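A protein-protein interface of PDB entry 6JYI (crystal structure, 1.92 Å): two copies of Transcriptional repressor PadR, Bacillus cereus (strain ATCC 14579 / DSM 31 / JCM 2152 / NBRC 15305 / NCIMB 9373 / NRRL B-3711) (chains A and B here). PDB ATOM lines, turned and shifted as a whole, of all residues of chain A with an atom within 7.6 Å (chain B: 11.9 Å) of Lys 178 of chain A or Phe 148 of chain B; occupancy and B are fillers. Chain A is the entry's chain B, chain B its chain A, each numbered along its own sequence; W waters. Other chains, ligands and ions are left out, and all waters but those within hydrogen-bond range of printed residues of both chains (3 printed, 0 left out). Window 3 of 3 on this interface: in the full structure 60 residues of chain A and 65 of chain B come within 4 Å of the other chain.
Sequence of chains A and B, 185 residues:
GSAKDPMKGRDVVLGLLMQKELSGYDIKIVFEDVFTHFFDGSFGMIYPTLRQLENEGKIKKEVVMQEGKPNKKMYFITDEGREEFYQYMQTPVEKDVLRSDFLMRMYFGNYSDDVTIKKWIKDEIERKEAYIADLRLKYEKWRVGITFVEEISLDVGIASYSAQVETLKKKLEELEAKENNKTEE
Among the printed residues, merely in contact across the chains: Glu 174 of chain A with Phe 148 of chain B, Lys 171 of chain A with Phe 148 of chain B, Asn 110 of chain A with Val 149 of chain B, Leu 168 of chain A with Ile 152 of chain B, Met 106 of chain A with Glu 150 of chain B, Lys 178 of chain A with Phe 148 of chain B, Met 106 of chain A with Ile 152 of chain B, Ile 121 of chain A with Ile 152 of chain B, Leu 168 of chain A with Val 156 of chain B, Ile 117 of chain A with Val 149 of chain B and Lys 171 of chain A with Ile 152 of chain B.
Of the 16 printed residues of chain B, 7 touch a printed residue of chain A. Hydrophobic or aromatic side chains of chain A that line the printed part of chain B: Met 106, Ile 117, Ile 121 and Leu 168. Among the printed residues, 15 pairs touch across the chains. Among the printed residues, Asp or Glu carboxylates within 4 Å of a Lys or Arg side-chain nitrogen of the other chain: Lys 171 of chain A with Asp 155 of chain B (2.7 Å).
The side-chain carboxylate (OE2) of Glu 151 of chain B lies close to the side-chain carboxylate (OD1) of Asp 155 of chain B (2.7 Å). O of Glu 150 of chain B lies within hydrogen-bond range of OG of Ser 153 of chain B (3.1 Å). The guanidinium group of Arg 143 of chain B lies within salt-bridge range of the side-chain carboxylate of Glu 150 of chain B, at 2.6 Å. N of Thr 147 of chain B sits at hydrogen-bond distance from OE1 of Glu 150 of chain B (3.0 Å).
No position is printed for both chains.
Of the printed residues of chain B, Ile 117 of chain A touches Val 149. Printed residues of chain B within 4 Å of Leu 168 of chain A: Ile 152 (3.7 Å) and Val 156 (3.9 Å). Lys 171 of chain A touches just these residues of chain B: Phe 148, Ile 152 and Asp 155. Glu 174 of chain A touches just one residue of chain B: Phe 148. No residue of chain B comes within 4 Å of Ala 177 of chain A. Lys 178 of chain A touches one residue of chain B. Tyr 139 of chain B touches none of the printed residues of chain A. Arg 143 of chain B touches none of the printed residues of chain A. Of the printed residues of chain A, Thr 147 of chain B touches Asn 110 (2.7 Å). Of chain A, only Lys 171, Glu 174 and Lys 178 come within 4 Å of Phe 148 of chain B. The nearest residue of chain B that does not touch Lys 178 of chain A is Val 149 of chain B (6.8 Å).
The side-chain carboxylate of Asp 155 of chain B is in salt-bridge range of the side-chain amino group of Lys 171 of chain A. The backbone carbonyl oxygen (O) of Met 106 of chain A sits close to the backbone carbonyl oxygen (O) of Val 149 of chain B (3.4 Å). The side-chain carboxylate (OE2) of Glu 150 of chain B sits at hydrogen-bond distance from the side-chain amide nitrogen (ND2) of Asn 110 of chain A, at 2.8 Å. The side-chain amide oxygen of Asn 110 of chain A lies within hydrogen-bond range of the side-chain hydroxyl of Thr 147 of chain B (2.7 Å).
Water W1 lies within hydrogen-bond range of the side-chain carboxylate of Glu 150 of chain B (2.6 Å), the backbone carbonyl oxygen of Gly 145 of chain B (2.8 Å), the guanidinium group of Arg 143 of chain B (3.3 Å) and the side-chain amide nitrogen of Asn 110 of chain A (3.4 Å). Water W2 bridges the side-chain amino group of Lys 171 of chain A (2.8 Å) and the backbone carbonyl oxygen of Phe 148 of chain B (2.9 Å). Water W3 lies within hydrogen-bond range of OE2 of Glu 150 of chain B (2.8 Å) and N of Asn 110 of chain A (3.0 Å).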
ATOM      1  N   MET A 106       5.354   5.113  16.641  1.00  0.00           N
ATOM      2  CA  MET A 106       6.638   4.417  16.849  1.00  0.00           C
ATOM      3  C   MET A 106       7.374   4.222  15.532  1.00  0.00           C
ATOM      4  O   MET A 106       8.547   4.526  15.443  1.00  0.00           O
ATOM      5  CB  MET A 106       6.424   3.068  17.502  1.00  0.00           C
ATOM      6  CG  MET A 106       5.847   3.124  18.916  1.00  0.00           C
ATOM      7  SD  MET A 106       6.787   4.134  20.291  1.00  0.00           S
ATOM      8  CE  MET A 106       5.889   5.836  20.138  1.00  0.00           C
ATOM      9  N   ASN A 110      11.437   8.420  14.537  1.00  0.00           N
ATOM     10  CA  ASN A 110      12.624   9.226  14.267  1.00  0.00           C
ATOM     11  C   ASN A 110      12.282  10.699  14.018  1.00  0.00           C
ATOM     12  O   ASN A 110      13.166  11.549  14.101  1.00  0.00           O
ATOM     13  CB  ASN A 110      13.442   8.662  13.100  1.00  0.00           C
ATOM     14  CG  ASN A 110      14.090   7.336  13.433  1.00  0.00           C
ATOM     15  OD1 ASN A 110      14.157   6.956  14.582  1.00  0.00           O
ATOM     16  ND2 ASN A 110      14.539   6.603  12.403  1.00  0.00           N
ATOM     17  N   ASP A 114      12.565  12.527  22.309  1.00  0.00           N
ATOM     18  CA  ASP A 114      12.546  11.607  23.448  1.00  0.00           C
ATOM     19  C   ASP A 114      11.426  11.914  24.416  1.00  0.00           C
ATOM     20  O   ASP A 114      10.780  11.007  24.931  1.00  0.00           O
ATOM     21  CB  ASP A 114      13.879  11.630  24.225  1.00  0.00           C
ATOM     22  CG  ASP A 114      14.902  10.647  23.692  1.00  0.00           C
ATOM     23  OD1 ASP A 114      14.840  10.283  22.504  1.00  0.00           O
ATOM     24  OD2 ASP A 114      15.820  10.290  24.473  1.00  0.00           O
ATOM     25  N   ILE A 117       8.109  10.717  22.821  1.00  0.00           N
ATOM     26  CA  ILE A 117       8.109   9.253  22.706  1.00  0.00           C
ATOM     27  C   ILE A 117       7.889   8.572  24.059  1.00  0.00           C
ATOM     28  O   ILE A 117       7.090   7.654  24.180  1.00  0.00           O
ATOM     29  CB  ILE A 117       9.389   8.731  22.011  1.00  0.00           C
ATOM     30  CG1 ILE A 117       9.378   9.116  20.510  1.00  0.00           C
ATOM     31  CG2 ILE A 117       9.540   7.184  22.233  1.00  0.00           C
ATOM     32  CD1 ILE A 117      10.734   9.046  19.782  1.00  0.00           C
ATOM     33  N   ILE A 121       4.694   6.239  25.168  1.00  0.00           N
ATOM     34  CA  ILE A 121       4.838   4.884  25.660  1.00  0.00           C
ATOM     35  C   ILE A 121       4.146   4.763  27.017  1.00  0.00           C
ATOM     36  O   ILE A 121       3.401   3.806  27.235  1.00  0.00           O
ATOM     37  CB  ILE A 121       6.309   4.439  25.726  1.00  0.00           C
ATOM     38  CG1 ILE A 121       6.941   4.416  24.344  1.00  0.00           C
ATOM     39  CG2 ILE A 121       6.455   3.042  26.417  1.00  0.00           C
ATOM     40  CD1 ILE A 121       8.470   4.375  24.394  1.00  0.00           C
ATOM     41  N   LEU A 168       6.285  -2.940  26.296  1.00  0.00           N
ATOM     42  CA  LEU A 168       6.393  -1.481  26.422  1.00  0.00           C
ATOM     43  C   LEU A 168       7.066  -1.025  27.725  1.00  0.00           C
ATOM     44  O   LEU A 168       7.826  -0.057  27.724  1.00  0.00           O
ATOM     45  CB  LEU A 168       5.032  -0.815  26.222  1.00  0.00           C
ATOM     46  CG  LEU A 168       4.515  -0.764  24.777  1.00  0.00           C
ATOM     47  CD1 LEU A 168       3.087  -0.214  24.694  1.00  0.00           C
ATOM     48  CD2 LEU A 168       5.427   0.055  23.842  1.00  0.00           C
ATOM     49  N   LYS A 170       9.427  -2.659  29.229  1.00  0.00           N
ATOM     50  CA  LYS A 170      10.853  -2.905  28.988  1.00  0.00           C
ATOM     51  C   LYS A 170      11.409  -1.818  28.098  1.00  0.00           C
ATOM     52  O   LYS A 170      12.509  -1.342  28.327  1.00  0.00           O
ATOM     53  CB  LYS A 170      11.100  -4.288  28.349  1.00  0.00           C
ATOM     54  CG  LYS A 170      10.859  -5.416  29.333  1.00  0.00           C
ATOM     55  CD  LYS A 170      11.031  -6.776  28.705  1.00  0.00           C
ATOM     56  CE  LYS A 170      11.107  -7.835  29.794  1.00  0.00           C
ATOM     57  NZ  LYS A 170      10.505  -9.109  29.327  1.00  0.00           N
ATOM     58  N   LYS A 171      10.651  -1.417  27.079  1.00  0.00           N
ATOM     59  CA  LYS A 171      11.093  -0.327  26.236  1.00  0.00           C
ATOM     60  C   LYS A 171      11.262   0.975  27.043  1.00  0.00           C
ATOM     61  O   LYS A 171      12.244   1.663  26.883  1.00  0.00           O
ATOM     62  CB  LYS A 171      10.131  -0.089  25.074  1.00  0.00           C
ATOM     63  CG  LYS A 171       9.955  -1.286  24.127  1.00  0.00           C
ATOM     64  CD  LYS A 171      11.287  -1.748  23.509  1.00  0.00           C
ATOM     65  CE  LYS A 171      11.082  -2.885  22.526  1.00  0.00           C
ATOM     66  NZ  LYS A 171      12.393  -3.347  21.936  1.00  0.00           N
ATOM     67  N   LEU A 172      10.287   1.316  27.890  1.00  0.00           N
ATOM     68  CA  LEU A 172      10.364   2.564  28.656  1.00  0.00           C
ATOM     69  C   LEU A 172      11.573   2.567  29.577  1.00  0.00           C
ATOM     70  O   LEU A 172      12.310   3.545  29.635  1.00  0.00           O
ATOM     71  CB  LEU A 172       9.064   2.777  29.446  1.00  0.00           C
ATOM     72  CG  LEU A 172       9.002   3.990  30.357  1.00  0.00           C
ATOM     73  CD1 LEU A 172       9.050   5.257  29.485  1.00  0.00           C
ATOM     74  CD2 LEU A 172       7.733   3.903  31.305  1.00  0.00           C
ATOM     75  N   GLU A 173      11.775   1.465  30.296  1.00  0.00           N
ATOM     76  CA  GLU A 173      12.925   1.300  31.166  1.00  0.00           C
ATOM     77  C   GLU A 173      14.219   1.469  30.371  1.00  0.00           C
ATOM     78  O   GLU A 173      15.159   2.116  30.815  1.00  0.00           O
ATOM     79  CB  GLU A 173      12.860  -0.086  31.842  1.00  0.00           C
ATOM     80  CG  GLU A 173      13.970  -0.387  32.787  1.00  0.00           C
ATOM     81  CD  GLU A 173      13.756  -1.693  33.573  1.00  0.00           C
ATOM     82  OE1 GLU A 173      14.768  -2.341  33.908  1.00  0.00           O
ATOM     83  OE2 GLU A 173      12.593  -2.074  33.841  1.00  0.00           O
ATOM     84  N   GLU A 174      14.287   0.888  29.190  1.00  0.00           N
ATOM     85  CA  GLU A 174      15.553   0.971  28.428  1.00  0.00           C
ATOM     86  C   GLU A 174      15.757   2.410  27.979  1.00  0.00           C
ATOM     87  O   GLU A 174      16.864   2.920  28.064  1.00  0.00           O
ATOM     88  CB  GLU A 174      15.551   0.047  27.217  1.00  0.00           C
ATOM     89  CG  GLU A 174      16.789   0.228  26.334  1.00  0.00           C
ATOM     90  CD  GLU A 174      16.871  -0.760  25.192  1.00  0.00           C
ATOM     91  OE1 GLU A 174      15.914  -1.535  24.996  1.00  0.00           O
ATOM     92  OE2 GLU A 174      17.919  -0.755  24.498  1.00  0.00           O
ATOM     93  N   LEU A 175      14.676   3.073  27.555  1.00  0.00           N
ATOM     94  CA  LEU A 175      14.739   4.470  27.129  1.00  0.00           C
ATOM     95  C   LEU A 175      15.151   5.379  28.277  1.00  0.00           C
ATOM     96  O   LEU A 175      16.010   6.244  28.120  1.00  0.00           O
ATOM     97  CB  LEU A 175      13.387   4.924  26.533  1.00  0.00           C
ATOM     98  CG  LEU A 175      13.323   6.356  26.021  1.00  0.00           C
ATOM     99  CD1 LEU A 175      14.540   6.658  25.122  1.00  0.00           C
ATOM    100  CD2 LEU A 175      12.020   6.573  25.199  1.00  0.00           C
ATOM    101  N   GLU A 176      14.566   5.166  29.442  1.00  0.00           N
ATOM    102  CA  GLU A 176      14.962   5.939  30.624  1.00  0.00           C
ATOM    103  C   GLU A 176      16.432   5.709  30.999  1.00  0.00           C
ATOM    104  O   GLU A 176      17.099   6.629  31.469  1.00  0.00           O
ATOM    105  CB  GLU A 176      14.029   5.629  31.797  1.00  0.00           C
ATOM    106  CG  GLU A 176      12.648   6.233  31.600  1.00  0.00           C
ATOM    107  CD  GLU A 176      11.623   5.764  32.605  1.00  0.00           C
ATOM    108  OE1 GLU A 176      11.867   4.790  33.342  1.00  0.00           O
ATOM    109  OE2 GLU A 176      10.539   6.371  32.653  1.00  0.00           O
ATOM    110  N   ALA A 177      16.939   4.494  30.776  1.00  0.00           N
ATOM    111  CA  ALA A 177      18.349   4.179  31.056  1.00  0.00           C
ATOM    112  C   ALA A 177      19.308   4.795  30.032  1.00  0.00           C
ATOM    113  O   ALA A 177      20.469   4.984  30.342  1.00  0.00           O
ATOM    114  CB  ALA A 177      18.583   2.659  31.170  1.00  0.00           C
ATOM    115  N   LYS A 178      18.828   5.095  28.826  1.00  0.00           N
ATOM    116  CA  LYS A 178      19.636   5.802  27.817  1.00  0.00           C
ATOM    117  C   LYS A 178      19.920   7.269  28.207  1.00  0.00           C
ATOM    118  O   LYS A 178      20.967   7.824  27.869  1.00  0.00           O
ATOM    119  CB  LYS A 178      18.923   5.828  26.459  1.00  0.00           C
ATOM    120  CG  LYS A 178      18.710   4.466  25.758  1.00  0.00           C
ATOM    121  CD  LYS A 178      18.157   4.691  24.338  1.00  0.00           C
ATOM    122  CE  LYS A 178      18.106   3.405  23.525  1.00  0.00           C
ATOM    123  NZ  LYS A 178      19.444   2.824  23.235  1.00  0.00           N
ATOM    124  N   GLU A 179      18.940   7.900  28.847  1.00  0.00           N
ATOM    125  CA  GLU A 179      19.029   9.293  29.268  1.00  0.00           C
ATOM    126  C   GLU A 179      19.548   9.345  30.705  1.00  0.00           C
ATOM    127  O   GLU A 179      20.751   9.151  30.944  1.00  0.00           O
ATOM    128  CB  GLU A 179      17.654   9.954  29.194  1.00  0.00           C
ATOM    129  CG  GLU A 179      16.860   9.661  27.893  1.00  0.00           C
ATOM    130  CD  GLU A 179      15.374   9.908  28.042  1.00  0.00           C
ATOM    131  OE1 GLU A 179      14.842   9.797  29.167  1.00  0.00           O
ATOM    132  OE2 GLU A 179      14.723  10.208  27.025  1.00  0.00           O
ATOM    133  N   TYR B 139      11.365  -5.855   8.085  1.00  0.00           N
ATOM    134  CA  TYR B 139      11.913  -4.636   8.723  1.00  0.00           C
ATOM    135  C   TYR B 139      13.391  -4.437   8.375  1.00  0.00           C
ATOM    136  O   TYR B 139      13.837  -3.324   8.199  1.00  0.00           O
ATOM    137  CB  TYR B 139      11.716  -4.657  10.243  1.00  0.00           C
ATOM    138  CG  TYR B 139      10.437  -4.043  10.739  1.00  0.00           C
ATOM    139  CD1 TYR B 139       9.213  -4.641  10.490  1.00  0.00           C
ATOM    140  CD2 TYR B 139      10.450  -2.873  11.474  1.00  0.00           C
ATOM    141  CE1 TYR B 139       8.041  -4.103  10.992  1.00  0.00           C
ATOM    142  CE2 TYR B 139       9.273  -2.308  11.960  1.00  0.00           C
ATOM    143  CZ  TYR B 139       8.077  -2.935  11.718  1.00  0.00           C
ATOM    144  OH  TYR B 139       6.915  -2.389  12.199  1.00  0.00           O
ATOM    145  N   ARG B 143      13.816  -0.957   6.775  1.00  0.00           N
ATOM    146  CA  ARG B 143      14.413  -0.040   7.736  1.00  0.00           C
ATOM    147  C   ARG B 143      15.863  -0.445   7.986  1.00  0.00           C
ATOM    148  O   ARG B 143      16.225  -0.936   9.070  1.00  0.00           O
ATOM    149  CB  ARG B 143      13.642  -0.038   9.056  1.00  0.00           C
ATOM    150  CG  ARG B 143      12.132   0.371   8.963  1.00  0.00           C
ATOM    151  CD  ARG B 143      11.963   1.868   8.983  1.00  0.00           C
ATOM    152  NE  ARG B 143      12.502   2.450   7.767  1.00  0.00           N
ATOM    153  CZ  ARG B 143      13.104   3.632   7.628  1.00  0.00           C
ATOM    154  NH1 ARG B 143      13.301   4.478   8.638  1.00  0.00           N
ATOM    155  NH2 ARG B 143      13.528   3.960   6.424  1.00  0.00           N
ATOM    156  N   VAL B 144      16.672  -0.256   6.960  1.00  0.00           N
ATOM    157  CA  VAL B 144      18.103  -0.356   7.119  1.00  0.00           C
ATOM    158  C   VAL B 144      18.442   0.898   7.944  1.00  0.00           C
ATOM    159  O   VAL B 144      17.975   2.027   7.672  1.00  0.00           O
ATOM    160  CB  VAL B 144      18.899  -0.450   5.774  1.00  0.00           C
ATOM    161  CG1 VAL B 144      18.153  -1.297   4.767  1.00  0.00           C
ATOM    162  CG2 VAL B 144      19.204   0.915   5.208  1.00  0.00           C
ATOM    163  N   GLY B 145      19.190   0.690   8.988  1.00  0.00           N
ATOM    164  CA  GLY B 145      19.483   1.760   9.900  1.00  0.00           C
ATOM    165  C   GLY B 145      18.403   1.858  10.951  1.00  0.00           C
ATOM    166  O   GLY B 145      18.271   2.891  11.569  1.00  0.00           O
ATOM    167  N   ILE B 146      17.661   0.775  11.184  1.00  0.00           N
ATOM    168  CA  ILE B 146      16.571   0.804  12.153  1.00  0.00           C
ATOM    169  C   ILE B 146      17.021   1.295  13.519  1.00  0.00           C
ATOM    170  O   ILE B 146      18.082   0.898  14.028  1.00  0.00           O
ATOM    171  CB  ILE B 146      15.868  -0.577  12.266  1.00  0.00           C
ATOM    172  CG1 ILE B 146      14.547  -0.405  13.003  1.00  0.00           C
ATOM    173  CG2 ILE B 146      16.792  -1.631  12.912  1.00  0.00           C
ATOM    174  CD1 ILE B 146      13.642  -1.591  12.949  1.00  0.00           C
ATOM    175  N   THR B 147      16.235   2.175  14.116  1.00  0.00           N
ATOM    176  CA  THR B 147      16.549   2.752  15.430  1.00  0.00           C
ATOM    177  C   THR B 147      15.706   2.161  16.544  1.00  0.00           C
ATOM    178  O   THR B 147      14.724   1.478  16.290  1.00  0.00           O
ATOM    179  CB  THR B 147      16.269   4.249  15.471  1.00  0.00           C
ATOM    180  OG1 THR B 147      14.868   4.473  15.302  1.00  0.00           O
ATOM    181  CG2 THR B 147      17.011   4.971  14.414  1.00  0.00           C
ATOM    182  N   PHE B 148      16.110   2.436  17.790  1.00  0.00           N
ATOM    183  CA  PHE B 148      15.401   1.954  18.963  1.00  0.00           C
ATOM    184  C   PHE B 148      13.886   2.183  18.854  1.00  0.00           C
ATOM    185  O   PHE B 148      13.116   1.255  19.068  1.00  0.00           O
ATOM    186  CB  PHE B 148      15.938   2.635  20.238  1.00  0.00           C
ATOM    187  CG  PHE B 148      15.109   2.380  21.463  1.00  0.00           C
ATOM    188  CD1 PHE B 148      15.351   1.264  22.245  1.00  0.00           C
ATOM    189  CD2 PHE B 148      14.084   3.224  21.823  1.00  0.00           C
ATOM    190  CE1 PHE B 148      14.571   1.009  23.386  1.00  0.00           C
ATOM    191  CE2 PHE B 148      13.318   2.973  22.942  1.00  0.00           C
ATOM    192  CZ  PHE B 148      13.555   1.876  23.721  1.00  0.00           C
ATOM    193  N   VAL B 149      13.448   3.392  18.508  1.00  0.00           N
ATOM    194  CA  VAL B 149      12.002   3.680  18.525  1.00  0.00           C
ATOM    195  C   VAL B 149      11.270   2.927  17.387  1.00  0.00           C
ATOM    196  O   VAL B 149      10.164   2.448  17.579  1.00  0.00           O
ATOM    197  CB  VAL B 149      11.690   5.165  18.469  1.00  0.00           C
ATOM    198  CG1 VAL B 149      12.308   5.809  17.247  1.00  0.00           C
ATOM    199  CG2 VAL B 149      10.153   5.420  18.534  1.00  0.00           C
ATOM    200  N   GLU B 150      11.891   2.864  16.217  1.00  0.00           N
ATOM    201  CA  GLU B 150      11.329   2.100  15.078  1.00  0.00           C
ATOM    202  C   GLU B 150      11.180   0.624  15.405  1.00  0.00           C
ATOM    203  O   GLU B 150      10.245  -0.038  14.958  1.00  0.00           O
ATOM    204  CB  GLU B 150      12.195   2.261  13.838  1.00  0.00           C
ATOM    205  CG  GLU B 150      12.193   3.703  13.300  1.00  0.00           C
ATOM    206  CD  GLU B 150      13.137   3.896  12.128  1.00  0.00           C
ATOM    207  OE1 GLU B 150      14.242   3.301  12.175  1.00  0.00           O
ATOM    208  OE2 GLU B 150      12.798   4.699  11.205  1.00  0.00           O
ATOM    209  N   GLU B 151      12.105   0.094  16.177  1.00  0.00           N
ATOM    210  CA  GLU B 151      12.044  -1.291  16.556  1.00  0.00           C
ATOM    211  C   GLU B 151      10.837  -1.577  17.480  1.00  0.00           C
ATOM    212  O   GLU B 151      10.365  -2.712  17.528  1.00  0.00           O
ATOM    213  CB  GLU B 151      13.364  -1.706  17.224  1.00  0.00           C
ATOM    214  CG  GLU B 151      13.431  -3.129  17.712  1.00  0.00           C
ATOM    215  CD  GLU B 151      13.873  -4.136  16.661  1.00  0.00           C
ATOM    216  OE1 GLU B 151      14.492  -3.710  15.665  1.00  0.00           O
ATOM    217  OE2 GLU B 151      13.633  -5.368  16.879  1.00  0.00           O
ATOM    218  N   ILE B 152      10.334  -0.558  18.213  1.00  0.00           N
ATOM    219  CA  ILE B 152       9.156  -0.792  19.089  1.00  0.00           C
ATOM    220  C   ILE B 152       7.961  -1.322  18.280  1.00  0.00           C
ATOM    221  O   ILE B 152       7.313  -2.282  18.707  1.00  0.00           O
ATOM    222  CB  ILE B 152       8.774   0.451  19.926  1.00  0.00           C
ATOM    223  CG1 ILE B 152       9.953   0.868  20.798  1.00  0.00           C
ATOM    224  CG2 ILE B 152       7.478   0.204  20.794  1.00  0.00           C
ATOM    225  CD1 ILE B 152       9.768   2.187  21.558  1.00  0.00           C
ATOM    226  N   SER B 153       7.693  -0.763  17.106  1.00  0.00           N
ATOM    227  CA  SER B 153       6.542  -1.237  16.305  1.00  0.00           C
ATOM    228  C   SER B 153       6.665  -2.702  15.970  1.00  0.00           C
ATOM    229  O   SER B 153       5.704  -3.452  16.098  1.00  0.00           O
ATOM    230  CB  SER B 153       6.275  -0.388  15.025  1.00  0.00           C
ATOM    231  OG  SER B 153       7.325  -0.422  14.091  1.00  0.00           O
ATOM    232  N   LEU B 154       7.860  -3.127  15.555  1.00  0.00           N
ATOM    233  CA  LEU B 154       8.123  -4.536  15.301  1.00  0.00           C
ATOM    234  C   LEU B 154       7.946  -5.397  16.525  1.00  0.00           C
ATOM    235  O   LEU B 154       7.233  -6.425  16.482  1.00  0.00           O
ATOM    236  CB  LEU B 154       9.552  -4.725  14.766  1.00  0.00           C
ATOM    237  CG  LEU B 154      10.100  -6.123  14.557  1.00  0.00           C
ATOM    238  CD1 LEU B 154       9.218  -6.910  13.563  1.00  0.00           C
ATOM    239  CD2 LEU B 154      11.603  -6.052  14.103  1.00  0.00           C
ATOM    240  N   ASP B 155       8.633  -5.032  17.603  1.00  0.00           N
ATOM    241  CA  ASP B 155       8.676  -5.902  18.788  1.00  0.00           C
ATOM    242  C   ASP B 155       7.310  -5.986  19.469  1.00  0.00           C
ATOM    243  O   ASP B 155       6.950  -7.021  20.002  1.00  0.00           O
ATOM    244  CB  ASP B 155       9.695  -5.408  19.786  1.00  0.00           C
ATOM    245  CG  ASP B 155      11.119  -5.546  19.274  1.00  0.00           C
ATOM    246  OD1 ASP B 155      11.297  -6.021  18.134  1.00  0.00           O
ATOM    247  OD2 ASP B 155      12.035  -5.178  20.022  1.00  0.00           O
ATOM    248  N   VAL B 156       6.554  -4.901  19.452  1.00  0.00           N
ATOM    249  CA  VAL B 156       5.201  -4.955  20.019  1.00  0.00           C
ATOM    250  C   VAL B 156       4.323  -5.901  19.202  1.00  0.00           C
ATOM    251  O   VAL B 156       3.597  -6.769  19.753  1.00  0.00           O
ATOM    252  CB  VAL B 156       4.600  -3.551  20.190  1.00  0.00           C
ATOM    253  CG1 VAL B 156       3.141  -3.604  20.648  1.00  0.00           C
ATOM    254  CG2 VAL B 156       5.418  -2.770  21.223  1.00  0.00           C
ATOM    255  N   GLY B 157       4.447  -5.810  17.883  1.00  0.00           N
ATOM    256  CA  GLY B 157       3.700  -6.684  17.003  1.00  0.00           C
ATOM    257  C   GLY B 157       3.994  -8.135  17.184  1.00  0.00           C
ATOM    258  O   GLY B 157       3.067  -8.940  17.328  1.00  0.00           O
HETATM  259  O   HOH W   1      16.060   4.258  10.525  1.00  0.00           O
HETATM  260  O   HOH W   2      13.521  -1.160  20.685  1.00  0.00           O
HETATM  261  O   HOH W   3      11.070   6.764  12.088  1.00  0.00           O
